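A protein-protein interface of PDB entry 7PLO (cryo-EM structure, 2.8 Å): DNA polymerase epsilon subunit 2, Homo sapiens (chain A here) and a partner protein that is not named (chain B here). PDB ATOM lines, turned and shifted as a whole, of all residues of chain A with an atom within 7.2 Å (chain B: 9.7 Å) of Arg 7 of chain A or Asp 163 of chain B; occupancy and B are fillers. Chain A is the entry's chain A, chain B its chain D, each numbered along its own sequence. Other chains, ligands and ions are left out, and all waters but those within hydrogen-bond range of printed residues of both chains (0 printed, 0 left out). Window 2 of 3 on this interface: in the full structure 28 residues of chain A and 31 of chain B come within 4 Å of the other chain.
The side-chain carboxylate (OD1) of Asp 163 of chain B lies within salt-bridge range of the guanidinium group (NE) of Arg 7 of chain A. OE1 of Glu 132 of chain B sits close to OG of Ser 12 of chain A. O of Asp 162 of chain B is in hydrogen-bond range of NH2 of Arg 7 of chain A, at 3.4 Å. The backbone carbonyl oxygen (O) of Ser 8 of chain A sits close to the side-chain carboxylate (OE2) of Glu 132 of chain B, at 3.5 Å. The side-chain carboxylate (OE1) of Glu 160 of chain B is in salt-bridge range of the guanidinium group (NH2) of Arg 7 of chain A, at 2.7 Å.
O of Ser 8 of chain A lies within hydrogen-bond range of OG of Ser 12 of chain A (2.7 Å). The side-chain carboxylate (OD2) of Asp 162 of chain B sits at hydrogen-bond distance from the side-chain hydroxyl (OG1) of Thr 165 of chain B (2.9 Å). The backbone carbonyl oxygen of Glu 4 of chain A sits at hydrogen-bond distance from the side-chain hydroxyl of Ser 8 of chain A (2.8 Å).
Glu 132 of chain B touches Arg 9 of chain A (OE2 to N, 3.5 Å). CA of Gly 23 of chain A touches OE2 of Glu 160 of chain B, at 3.2 Å. Ile 26 of chain A touches Glu 160 of chain B.
Arg 7 of chain A touches three residues of chain B. Of chain A, only Arg 7 comes within 4 Å of Asp 163 of chain B. No residue of chain B comes within 4 Å of Leu 6 of chain A. Of chain B, only Glu 132 (3.2 Å) comes within 4 Å of Ser 8 of chain A. Ala 10 of chain A touches none of the printed residues of chain B. Of the printed residues of chain B, Ile 26 of chain A touches Glu 160 (3.7 Å). Of the printed residues of chain A, Glu 132 of chain B touches Ser 8 (3.2 Å), Arg 9 (3.5 Å) and Ser 12 (3.2 Å). Printed residues of chain B within 4 Å of Ser 12 of chain A: Glu 132. Of the printed residues of chain A, Asp 162 of chain B touches Arg 7 (3.4 Å). Printed residues of chain B within 4 Å of Arg 9 of chain A: Glu 132. Leu 21 of chain A touches none of the printed residues of chain B. The nearest residue of chain B that does not touch Arg 7 of chain A is Gly 164 of chain B (5.4 Å). The nearest printed residue of chain B that does not touch Gly 23 of chain A is Phe 159 of chain B (6.4 Å).
Of the 11 printed residues of chain B, 4 touch a printed residue of chain A. Of the 21 printed residues of chain A, 6 touch a printed residue of chain B. Printed residues of chain A that touch a printed residue of chain B: Arg 7, Ser 8, Arg 9, Ser 12, Gly 23 and Ile 26. Hydrophobic or aromatic side chains of chain A within 4 Å of the printed part of chain B: Ile 26. Among the printed residues, 8 pairs touch across the chains. Among the printed residues, Asp or Glu carboxylates within 4 Å of a Lys or Arg side-chain nitrogen of the other chain: Arg 7 of chain A with Glu 160 of chain B (2.7 Å) and Arg 7 of chain A with Asp 163 of chain B (3.2 Å).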
ATOM      1  N   ALA A   2     -30.100   4.984 -12.144  1.00  0.00           N
ATOM      2  CA  ALA A   2     -29.611   6.018 -11.241  1.00  0.00           C
ATOM      3  C   ALA A   2     -30.016   7.413 -11.741  1.00  0.00           C
ATOM      4  O   ALA A   2     -29.924   7.694 -12.952  1.00  0.00           O
ATOM      5  CB  ALA A   2     -28.094   5.944 -11.109  1.00  0.00           C
ATOM      6  N   PRO A   3     -30.469   8.317 -10.856  1.00  0.00           N
ATOM      7  CA  PRO A   3     -30.824   9.663 -11.332  1.00  0.00           C
ATOM      8  C   PRO A   3     -29.640  10.421 -11.897  1.00  0.00           C
ATOM      9  O   PRO A   3     -29.817  11.249 -12.799  1.00  0.00           O
ATOM     10  CB  PRO A   3     -31.388  10.338 -10.075  1.00  0.00           C
ATOM     11  CG  PRO A   3     -30.675   9.687  -8.966  1.00  0.00           C
ATOM     12  CD  PRO A   3     -30.514   8.255  -9.380  1.00  0.00           C
ATOM     13  N   GLU A   4     -28.433  10.159 -11.394  1.00  0.00           N
ATOM     14  CA  GLU A   4     -27.248  10.776 -11.976  1.00  0.00           C
ATOM     15  C   GLU A   4     -27.029  10.297 -13.407  1.00  0.00           C
ATOM     16  O   GLU A   4     -26.624  11.082 -14.270  1.00  0.00           O
ATOM     17  CB  GLU A   4     -26.022  10.482 -11.110  1.00  0.00           C
ATOM     18  CG  GLU A   4     -24.758  11.216 -11.549  1.00  0.00           C
ATOM     19  CD  GLU A   4     -23.602  11.017 -10.588  1.00  0.00           C
ATOM     20  OE1 GLU A   4     -23.788  10.328  -9.564  1.00  0.00           O
ATOM     21  OE2 GLU A   4     -22.507  11.552 -10.858  1.00  0.00           O
ATOM     22  N   ARG A   5     -27.287   9.014 -13.678  1.00  0.00           N
ATOM     23  CA  ARG A   5     -27.192   8.519 -15.048  1.00  0.00           C
ATOM     24  C   ARG A   5     -28.220   9.193 -15.951  1.00  0.00           C
ATOM     25  O   ARG A   5     -27.909   9.564 -17.095  1.00  0.00           O
ATOM     26  CB  ARG A   5     -27.370   7.000 -15.073  1.00  0.00           C
ATOM     27  CG  ARG A   5     -26.205   6.224 -14.471  1.00  0.00           C
ATOM     28  CD  ARG A   5     -26.461   4.719 -14.482  1.00  0.00           C
ATOM     29  NE  ARG A   5     -25.424   3.979 -13.767  1.00  0.00           N
ATOM     30  CZ  ARG A   5     -25.410   2.664 -13.585  1.00  0.00           C
ATOM     31  NH1 ARG A   5     -26.372   1.881 -14.053  1.00  0.00           N
ATOM     32  NH2 ARG A   5     -24.401   2.115 -12.913  1.00  0.00           N
ATOM     33  N   LEU A   6     -29.453   9.360 -15.454  1.00  0.00           N
ATOM     34  CA  LEU A   6     -30.463  10.061 -16.248  1.00  0.00           C
ATOM     35  C   LEU A   6     -30.043  11.502 -16.527  1.00  0.00           C
ATOM     36  O   LEU A   6     -30.193  11.995 -17.655  1.00  0.00           O
ATOM     37  CB  LEU A   6     -31.820  10.023 -15.537  1.00  0.00           C
ATOM     38  CG  LEU A   6     -32.986  10.798 -16.172  1.00  0.00           C
ATOM     39  CD1 LEU A   6     -33.236  10.376 -17.616  1.00  0.00           C
ATOM     40  CD2 LEU A   6     -34.252  10.621 -15.348  1.00  0.00           C
ATOM     41  N   ARG A   7     -29.510  12.189 -15.510  1.00  0.00           N
ATOM     42  CA  ARG A   7     -29.000  13.545 -15.693  1.00  0.00           C
ATOM     43  C   ARG A   7     -27.893  13.573 -16.738  1.00  0.00           C
ATOM     44  O   ARG A   7     -27.858  14.467 -17.593  1.00  0.00           O
ATOM     45  CB  ARG A   7     -28.486  14.090 -14.354  1.00  0.00           C
ATOM     46  CG  ARG A   7     -27.870  15.503 -14.395  1.00  0.00           C
ATOM     47  CD  ARG A   7     -27.288  15.913 -13.050  1.00  0.00           C
ATOM     48  NE  ARG A   7     -26.311  16.991 -13.200  1.00  0.00           N
ATOM     49  CZ  ARG A   7     -26.575  18.293 -13.176  1.00  0.00           C
ATOM     50  NH1 ARG A   7     -27.798  18.759 -12.967  1.00  0.00           N
ATOM     51  NH2 ARG A   7     -25.583  19.156 -13.371  1.00  0.00           N
ATOM     52  N   SER A   8     -26.971  12.611 -16.667  1.00  0.00           N
ATOM     53  CA  SER A   8     -25.835  12.586 -17.579  1.00  0.00           C
ATOM     54  C   SER A   8     -26.297  12.441 -19.019  1.00  0.00           C
ATOM     55  O   SER A   8     -25.839  13.172 -19.903  1.00  0.00           O
ATOM     56  CB  SER A   8     -24.887  11.448 -17.200  1.00  0.00           C
ATOM     57  OG  SER A   8     -24.438  11.581 -15.863  1.00  0.00           O
ATOM     58  N   ARG A   9     -27.233  11.523 -19.274  1.00  0.00           N
ATOM     59  CA  ARG A   9     -27.673  11.334 -20.655  1.00  0.00           C
ATOM     60  C   ARG A   9     -28.541  12.489 -21.143  1.00  0.00           C
ATOM     61  O   ARG A   9     -28.464  12.851 -22.324  1.00  0.00           O
ATOM     62  CB  ARG A   9     -28.401  10.000 -20.810  1.00  0.00           C
ATOM     63  CG  ARG A   9     -27.461   8.804 -20.733  1.00  0.00           C
ATOM     64  CD  ARG A   9     -27.921   7.634 -21.580  1.00  0.00           C
ATOM     65  NE  ARG A   9     -26.946   6.549 -21.522  1.00  0.00           N
ATOM     66  CZ  ARG A   9     -27.109   5.339 -22.044  1.00  0.00           C
ATOM     67  NH1 ARG A   9     -28.213   4.999 -22.693  1.00  0.00           N
ATOM     68  NH2 ARG A   9     -26.137   4.442 -21.908  1.00  0.00           N
ATOM     69  N   ALA A  10     -29.354  13.093 -20.270  1.00  0.00           N
ATOM     70  CA  ALA A  10     -30.126  14.266 -20.679  1.00  0.00           C
ATOM     71  C   ALA A  10     -29.204  15.419 -21.069  1.00  0.00           C
ATOM     72  O   ALA A  10     -29.374  16.051 -22.128  1.00  0.00           O
ATOM     73  CB  ALA A  10     -31.063  14.684 -19.547  1.00  0.00           C
ATOM     74  N   LEU A  11     -28.204  15.694 -20.223  1.00  0.00           N
ATOM     75  CA  LEU A  11     -27.235  16.740 -20.520  1.00  0.00           C
ATOM     76  C   LEU A  11     -26.463  16.426 -21.792  1.00  0.00           C
ATOM     77  O   LEU A  11     -26.211  17.320 -22.604  1.00  0.00           O
ATOM     78  CB  LEU A  11     -26.268  16.909 -19.349  1.00  0.00           C
ATOM     79  CG  LEU A  11     -26.786  17.566 -18.069  1.00  0.00           C
ATOM     80  CD1 LEU A  11     -25.753  17.426 -16.969  1.00  0.00           C
ATOM     81  CD2 LEU A  11     -27.107  19.030 -18.291  1.00  0.00           C
ATOM     82  N   SER A  12     -26.072  15.162 -21.978  1.00  0.00           N
ATOM     83  CA  SER A  12     -25.319  14.786 -23.168  1.00  0.00           C
ATOM     84  C   SER A  12     -26.146  14.981 -24.431  1.00  0.00           C
ATOM     85  O   SER A  12     -25.628  15.447 -25.449  1.00  0.00           O
ATOM     86  CB  SER A  12     -24.851  13.338 -23.051  1.00  0.00           C
ATOM     87  OG  SER A  12     -23.993  13.172 -21.936  1.00  0.00           O
ATOM     88  N   ALA A  13     -27.434  14.628 -24.388  1.00  0.00           N
ATOM     89  CA  ALA A  13     -28.287  14.816 -25.557  1.00  0.00           C
ATOM     90  C   ALA A  13     -28.412  16.292 -25.913  1.00  0.00           C
ATOM     91  O   ALA A  13     -28.201  16.686 -27.071  1.00  0.00           O
ATOM     92  CB  ALA A  13     -29.664  14.204 -25.302  1.00  0.00           C
ATOM     93  N   LEU A  21     -28.489  23.660 -20.597  1.00  0.00           N
ATOM     94  CA  LEU A  21     -29.630  23.713 -19.693  1.00  0.00           C
ATOM     95  C   LEU A  21     -29.266  24.482 -18.431  1.00  0.00           C
ATOM     96  O   LEU A  21     -28.182  24.296 -17.870  1.00  0.00           O
ATOM     97  CB  LEU A  21     -30.090  22.305 -19.310  1.00  0.00           C
ATOM     98  CG  LEU A  21     -30.692  21.417 -20.401  1.00  0.00           C
ATOM     99  CD1 LEU A  21     -30.878  20.007 -19.876  1.00  0.00           C
ATOM    100  CD2 LEU A  21     -32.018  21.969 -20.890  1.00  0.00           C
ATOM    101  N   ARG A  22     -30.176  25.345 -17.987  1.00  0.00           N
ATOM    102  CA  ARG A  22     -30.042  25.932 -16.664  1.00  0.00           C
ATOM    103  C   ARG A  22     -30.152  24.836 -15.607  1.00  0.00           C
ATOM    104  O   ARG A  22     -30.629  23.726 -15.872  1.00  0.00           O
ATOM    105  CB  ARG A  22     -31.115  26.995 -16.426  1.00  0.00           C
ATOM    106  CG  ARG A  22     -30.954  28.272 -17.245  1.00  0.00           C
ATOM    107  CD  ARG A  22     -30.015  29.294 -16.607  1.00  0.00           C
ATOM    108  NE  ARG A  22     -30.224  30.603 -17.223  1.00  0.00           N
ATOM    109  CZ  ARG A  22     -29.289  31.429 -17.680  1.00  0.00           C
ATOM    110  NH1 ARG A  22     -27.995  31.211 -17.486  1.00  0.00           N
ATOM    111  NH2 ARG A  22     -29.661  32.513 -18.355  1.00  0.00           N
ATOM    112  N   GLY A  23     -29.691  25.157 -14.397  1.00  0.00           N
ATOM    113  CA  GLY A  23     -29.713  24.170 -13.327  1.00  0.00           C
ATOM    114  C   GLY A  23     -31.120  23.729 -12.973  1.00  0.00           C
ATOM    115  O   GLY A  23     -31.402  22.530 -12.860  1.00  0.00           O
ATOM    116  N   ILE A  26     -32.481  21.446 -15.901  1.00  0.00           N
ATOM    117  CA  ILE A  26     -32.052  20.049 -15.882  1.00  0.00           C
ATOM    118  C   ILE A  26     -32.634  19.327 -14.673  1.00  0.00           C
ATOM    119  O   ILE A  26     -32.908  18.125 -14.744  1.00  0.00           O
ATOM    120  CB  ILE A  26     -30.510  19.922 -15.941  1.00  0.00           C
ATOM    121  CG1 ILE A  26     -30.047  18.450 -15.947  1.00  0.00           C
ATOM    122  CG2 ILE A  26     -29.831  20.619 -14.763  1.00  0.00           C
ATOM    123  CD1 ILE A  26     -30.625  17.571 -17.053  1.00  0.00           C
ATOM    124  N   LYS A  27     -32.819  20.026 -13.547  1.00  0.00           N
ATOM    125  CA  LYS A  27     -33.463  19.400 -12.394  1.00  0.00           C
ATOM    126  C   LYS A  27     -34.893  18.976 -12.729  1.00  0.00           C
ATOM    127  O   LYS A  27     -35.316  17.844 -12.427  1.00  0.00           O
ATOM    128  CB  LYS A  27     -33.434  20.375 -11.216  1.00  0.00           C
ATOM    129  CG  LYS A  27     -33.745  19.759  -9.868  1.00  0.00           C
ATOM    130  CD  LYS A  27     -33.441  20.734  -8.739  1.00  0.00           C
ATOM    131  CE  LYS A  27     -33.841  20.168  -7.386  1.00  0.00           C
ATOM    132  NZ  LYS A  27     -33.083  18.932  -7.044  1.00  0.00           N
ATOM    133  N   LEU A  29     -36.033  18.326 -15.742  1.00  0.00           N
ATOM    134  CA  LEU A  29     -35.992  17.248 -16.725  1.00  0.00           C
ATOM    135  C   LEU A  29     -35.660  15.909 -16.073  1.00  0.00           C
ATOM    136  O   LEU A  29     -36.302  14.886 -16.367  1.00  0.00           O
ATOM    137  CB  LEU A  29     -34.972  17.597 -17.809  1.00  0.00           C
ATOM    138  CG  LEU A  29     -34.854  16.720 -19.055  1.00  0.00           C
ATOM    139  CD1 LEU A  29     -36.161  16.651 -19.825  1.00  0.00           C
ATOM    140  CD2 LEU A  29     -33.749  17.272 -19.940  1.00  0.00           C
ATOM    141  N   THR A  30     -34.674  15.896 -15.171  1.00  0.00           N
ATOM    142  CA  THR A  30     -34.203  14.656 -14.575  1.00  0.00           C
ATOM    143  C   THR A  30     -35.130  14.124 -13.493  1.00  0.00           C
ATOM    144  O   THR A  30     -34.909  12.996 -13.040  1.00  0.00           O
ATOM    145  CB  THR A  30     -32.786  14.828 -14.001  1.00  0.00           C
ATOM    146  OG1 THR A  30     -32.238  13.543 -13.680  1.00  0.00           O
ATOM    147  CG2 THR A  30     -32.780  15.694 -12.745  1.00  0.00           C
ATOM    148  N   GLN A  34     -38.189  10.320 -14.897  1.00  0.00           N
ATOM    149  CA  GLN A  34     -37.871   9.154 -14.076  1.00  0.00           C
ATOM    150  C   GLN A  34     -38.679   7.923 -14.472  1.00  0.00           C
ATOM    151  O   GLN A  34     -38.231   6.799 -14.217  1.00  0.00           O
ATOM    152  CB  GLN A  34     -38.103   9.468 -12.595  1.00  0.00           C
ATOM    153  CG  GLN A  34     -37.030  10.349 -11.965  1.00  0.00           C
ATOM    154  CD  GLN A  34     -35.695   9.637 -11.809  1.00  0.00           C
ATOM    155  OE1 GLN A  34     -35.628   8.408 -11.812  1.00  0.00           O
ATOM    156  NE2 GLN A  34     -34.625  10.411 -11.680  1.00  0.00           N
ATOM    157  N   LEU A  41     -35.127   5.866 -23.786  1.00  0.00           N
ATOM    158  CA  LEU A  41     -34.758   7.164 -23.226  1.00  0.00           C
ATOM    159  C   LEU A  41     -34.224   8.110 -24.293  1.00  0.00           C
ATOM    160  O   LEU A  41     -34.532   9.308 -24.275  1.00  0.00           O
ATOM    161  CB  LEU A  41     -33.726   6.981 -22.110  1.00  0.00           C
ATOM    162  CG  LEU A  41     -33.145   8.244 -21.454  1.00  0.00           C
ATOM    163  CD1 LEU A  41     -34.235   9.161 -20.908  1.00  0.00           C
ATOM    164  CD2 LEU A  41     -32.172   7.865 -20.349  1.00  0.00           C
ATOM    165  N   GLU B 132     -23.361   8.349 -24.928  1.00  0.00           N
ATOM    166  CA  GLU B 132     -23.243   9.803 -24.816  1.00  0.00           C
ATOM    167  C   GLU B 132     -22.320  10.421 -25.866  1.00  0.00           C
ATOM    168  O   GLU B 132     -22.043  11.626 -25.794  1.00  0.00           O
ATOM    169  CB  GLU B 132     -22.784  10.234 -23.417  1.00  0.00           C
ATOM    170  CG  GLU B 132     -23.728   9.800 -22.308  1.00  0.00           C
ATOM    171  CD  GLU B 132     -23.281  10.270 -20.939  1.00  0.00           C
ATOM    172  OE1 GLU B 132     -22.132  10.742 -20.814  1.00  0.00           O
ATOM    173  OE2 GLU B 132     -24.083  10.168 -19.986  1.00  0.00           O
ATOM    174  N   PHE B 159     -24.730  29.241 -14.320  1.00  0.00           N
ATOM    175  CA  PHE B 159     -24.102  28.244 -15.183  1.00  0.00           C
ATOM    176  C   PHE B 159     -23.581  27.128 -14.287  1.00  0.00           C
ATOM    177  O   PHE B 159     -22.711  27.369 -13.442  1.00  0.00           O
ATOM    178  CB  PHE B 159     -22.985  28.886 -16.007  1.00  0.00           C
ATOM    179  CG  PHE B 159     -22.174  27.917 -16.813  1.00  0.00           C
ATOM    180  CD1 PHE B 159     -22.720  27.273 -17.910  1.00  0.00           C
ATOM    181  CD2 PHE B 159     -20.852  27.677 -16.491  1.00  0.00           C
ATOM    182  CE1 PHE B 159     -21.965  26.391 -18.653  1.00  0.00           C
ATOM    183  CE2 PHE B 159     -20.094  26.800 -17.232  1.00  0.00           C
ATOM    184  CZ  PHE B 159     -20.650  26.156 -18.315  1.00  0.00           C
ATOM    185  N   GLU B 160     -24.143  25.929 -14.441  1.00  0.00           N
ATOM    186  CA  GLU B 160     -23.762  24.809 -13.591  1.00  0.00           C
ATOM    187  C   GLU B 160     -22.398  24.270 -13.986  1.00  0.00           C
ATOM    188  O   GLU B 160     -22.068  24.184 -15.172  1.00  0.00           O
ATOM    189  CB  GLU B 160     -24.791  23.682 -13.677  1.00  0.00           C
ATOM    190  CG  GLU B 160     -26.020  23.887 -12.815  1.00  0.00           C
ATOM    191  CD  GLU B 160     -26.767  22.596 -12.556  1.00  0.00           C
ATOM    192  OE1 GLU B 160     -26.580  21.630 -13.326  1.00  0.00           O
ATOM    193  OE2 GLU B 160     -27.546  22.548 -11.582  1.00  0.00           O
ATOM    194  N   VAL B 161     -21.612  23.895 -12.973  1.00  0.00           N
ATOM    195  CA  VAL B 161     -20.273  23.351 -13.168  1.00  0.00           C
ATOM    196  C   VAL B 161     -20.160  21.925 -12.642  1.00  0.00           C
ATOM    197  O   VAL B 161     -19.470  21.094 -13.242  1.00  0.00           O
ATOM    198  CB  VAL B 161     -19.186  24.264 -12.547  1.00  0.00           C
ATOM    199  CG1 VAL B 161     -19.214  25.646 -13.220  1.00  0.00           C
ATOM    200  CG2 VAL B 161     -19.329  24.391 -11.036  1.00  0.00           C
ATOM    201  N   ASP B 162     -20.828  21.619 -11.531  1.00  0.00           N
ATOM    202  CA  ASP B 162     -21.006  20.264 -11.021  1.00  0.00           C
ATOM    203  C   ASP B 162     -22.504  19.993 -10.887  1.00  0.00           C
ATOM    204  O   ASP B 162     -23.340  20.765 -11.365  1.00  0.00           O
ATOM    205  CB  ASP B 162     -20.282  20.068  -9.686  1.00  0.00           C
ATOM    206  CG  ASP B 162     -18.867  20.611  -9.699  1.00  0.00           C
ATOM    207  OD1 ASP B 162     -18.187  20.477 -10.737  1.00  0.00           O
ATOM    208  OD2 ASP B 162     -18.433  21.169  -8.669  1.00  0.00           O
ATOM    209  N   ASP B 163     -22.836  18.870 -10.244  1.00  0.00           N
ATOM    210  CA  ASP B 163     -24.235  18.487 -10.081  1.00  0.00           C
ATOM    211  C   ASP B 163     -25.005  19.524  -9.270  1.00  0.00           C
ATOM    212  O   ASP B 163     -26.071  19.990  -9.690  1.00  0.00           O
ATOM    213  CB  ASP B 163     -24.317  17.112  -9.415  1.00  0.00           C
ATOM    214  CG  ASP B 163     -25.734  16.562  -9.366  1.00  0.00           C
ATOM    215  OD1 ASP B 163     -26.631  17.136 -10.018  1.00  0.00           O
ATOM    216  OD2 ASP B 163     -25.949  15.547  -8.671  1.00  0.00           O
ATOM    217  N   GLY B 164     -24.472  19.905  -8.110  1.00  0.00           N
ATOM    218  CA  GLY B 164     -25.122  20.818  -7.194  1.00  0.00           C
ATOM    219  C   GLY B 164     -24.597  22.236  -7.168  1.00  0.00           C
ATOM    220  O   GLY B 164     -25.111  23.043  -6.385  1.00  0.00           O
ATOM    221  N   THR B 165     -23.606  22.572  -7.998  1.00  0.00           N
ATOM    222  CA  THR B 165     -22.900  23.845  -7.928  1.00  0.00           C
ATOM    223  C   THR B 165     -23.018  24.613  -9.239  1.00  0.00           C
ATOM    224  O   THR B 165     -22.993  24.034 -10.333  1.00  0.00           O
ATOM    225  CB  THR B 165     -21.413  23.645  -7.605  1.00  0.00           C
ATOM    226  OG1 THR B 165     -20.782  22.936  -8.673  1.00  0.00           O
ATOM    227  CG2 THR B 165     -21.226  22.866  -6.311  1.00  0.00           C
ATOM    228  N   SER B 166     -23.102  25.936  -9.111  1.00  0.00           N
ATOM    229  CA  SER B 166     -23.189  26.826 -10.256  1.00  0.00           C
ATOM    230  C   SER B 166     -22.490  28.134  -9.923  1.00  0.00           C
ATOM    231  O   SER B 166     -22.281  28.471  -8.755  1.00  0.00           O
ATOM    232  CB  SER B 166     -24.643  27.094 -10.657  1.00  0.00           C
ATOM    233  OG  SER B 166     -25.398  27.554  -9.551  1.00  0.00           O
ATOM    234  N   TRP B 180     -12.778  22.769 -20.552  1.00  0.00           N
ATOM    235  CA  TRP B 180     -13.781  22.070 -21.346  1.00  0.00           C
ATOM    236  C   TRP B 180     -15.189  22.549 -21.020  1.00  0.00           C
ATOM    237  O   TRP B 180     -16.073  22.489 -21.881  1.00  0.00           O
ATOM    238  CB  TRP B 180     -13.655  20.554 -21.153  1.00  0.00           C
ATOM    239  CG  TRP B 180     -13.925  20.023 -19.766  1.00  0.00           C
ATOM    240  CD1 TRP B 180     -13.036  19.932 -18.734  1.00  0.00           C
ATOM    241  CD2 TRP B 180     -15.156  19.466 -19.281  1.00  0.00           C
ATOM    242  NE1 TRP B 180     -13.639  19.370 -17.634  1.00  0.00           N
ATOM    243  CE2 TRP B 180     -14.941  19.076 -17.943  1.00  0.00           C
ATOM    244  CE3 TRP B 180     -16.421  19.268 -19.844  1.00  0.00           C
ATOM    245  CZ2 TRP B 180     -15.941  18.502 -17.162  1.00  0.00           C
ATOM    246  CZ3 TRP B 180     -17.415  18.699 -19.065  1.00  0.00           C
ATOM    247  CH2 TRP B 180     -17.168  18.322 -17.739  1.00  0.00           C
ATOM    248  N   LYS B 181     -15.414  23.036 -19.799  1.00  0.00           N
ATOM    249  CA  LYS B 181     -16.695  23.655 -19.475  1.00  0.00           C
ATOM    250  C   LYS B 181     -16.817  25.048 -20.082  1.00  0.00           C
ATOM    251  O   LYS B 181     -17.889  25.418 -20.571  1.00  0.00           O
ATOM    252  CB  LYS B 181     -16.892  23.725 -17.954  1.00  0.00           C
ATOM    253  CG  LYS B 181     -17.569  22.506 -17.299  1.00  0.00           C
ATOM    254  CD  LYS B 181     -18.989  22.278 -17.827  1.00  0.00           C
ATOM    255  CE  LYS B 181     -19.902  21.576 -16.838  1.00  0.00           C
ATOM    256  NZ  LYS B 181     -19.465  20.212 -16.454  1.00  0.00           N
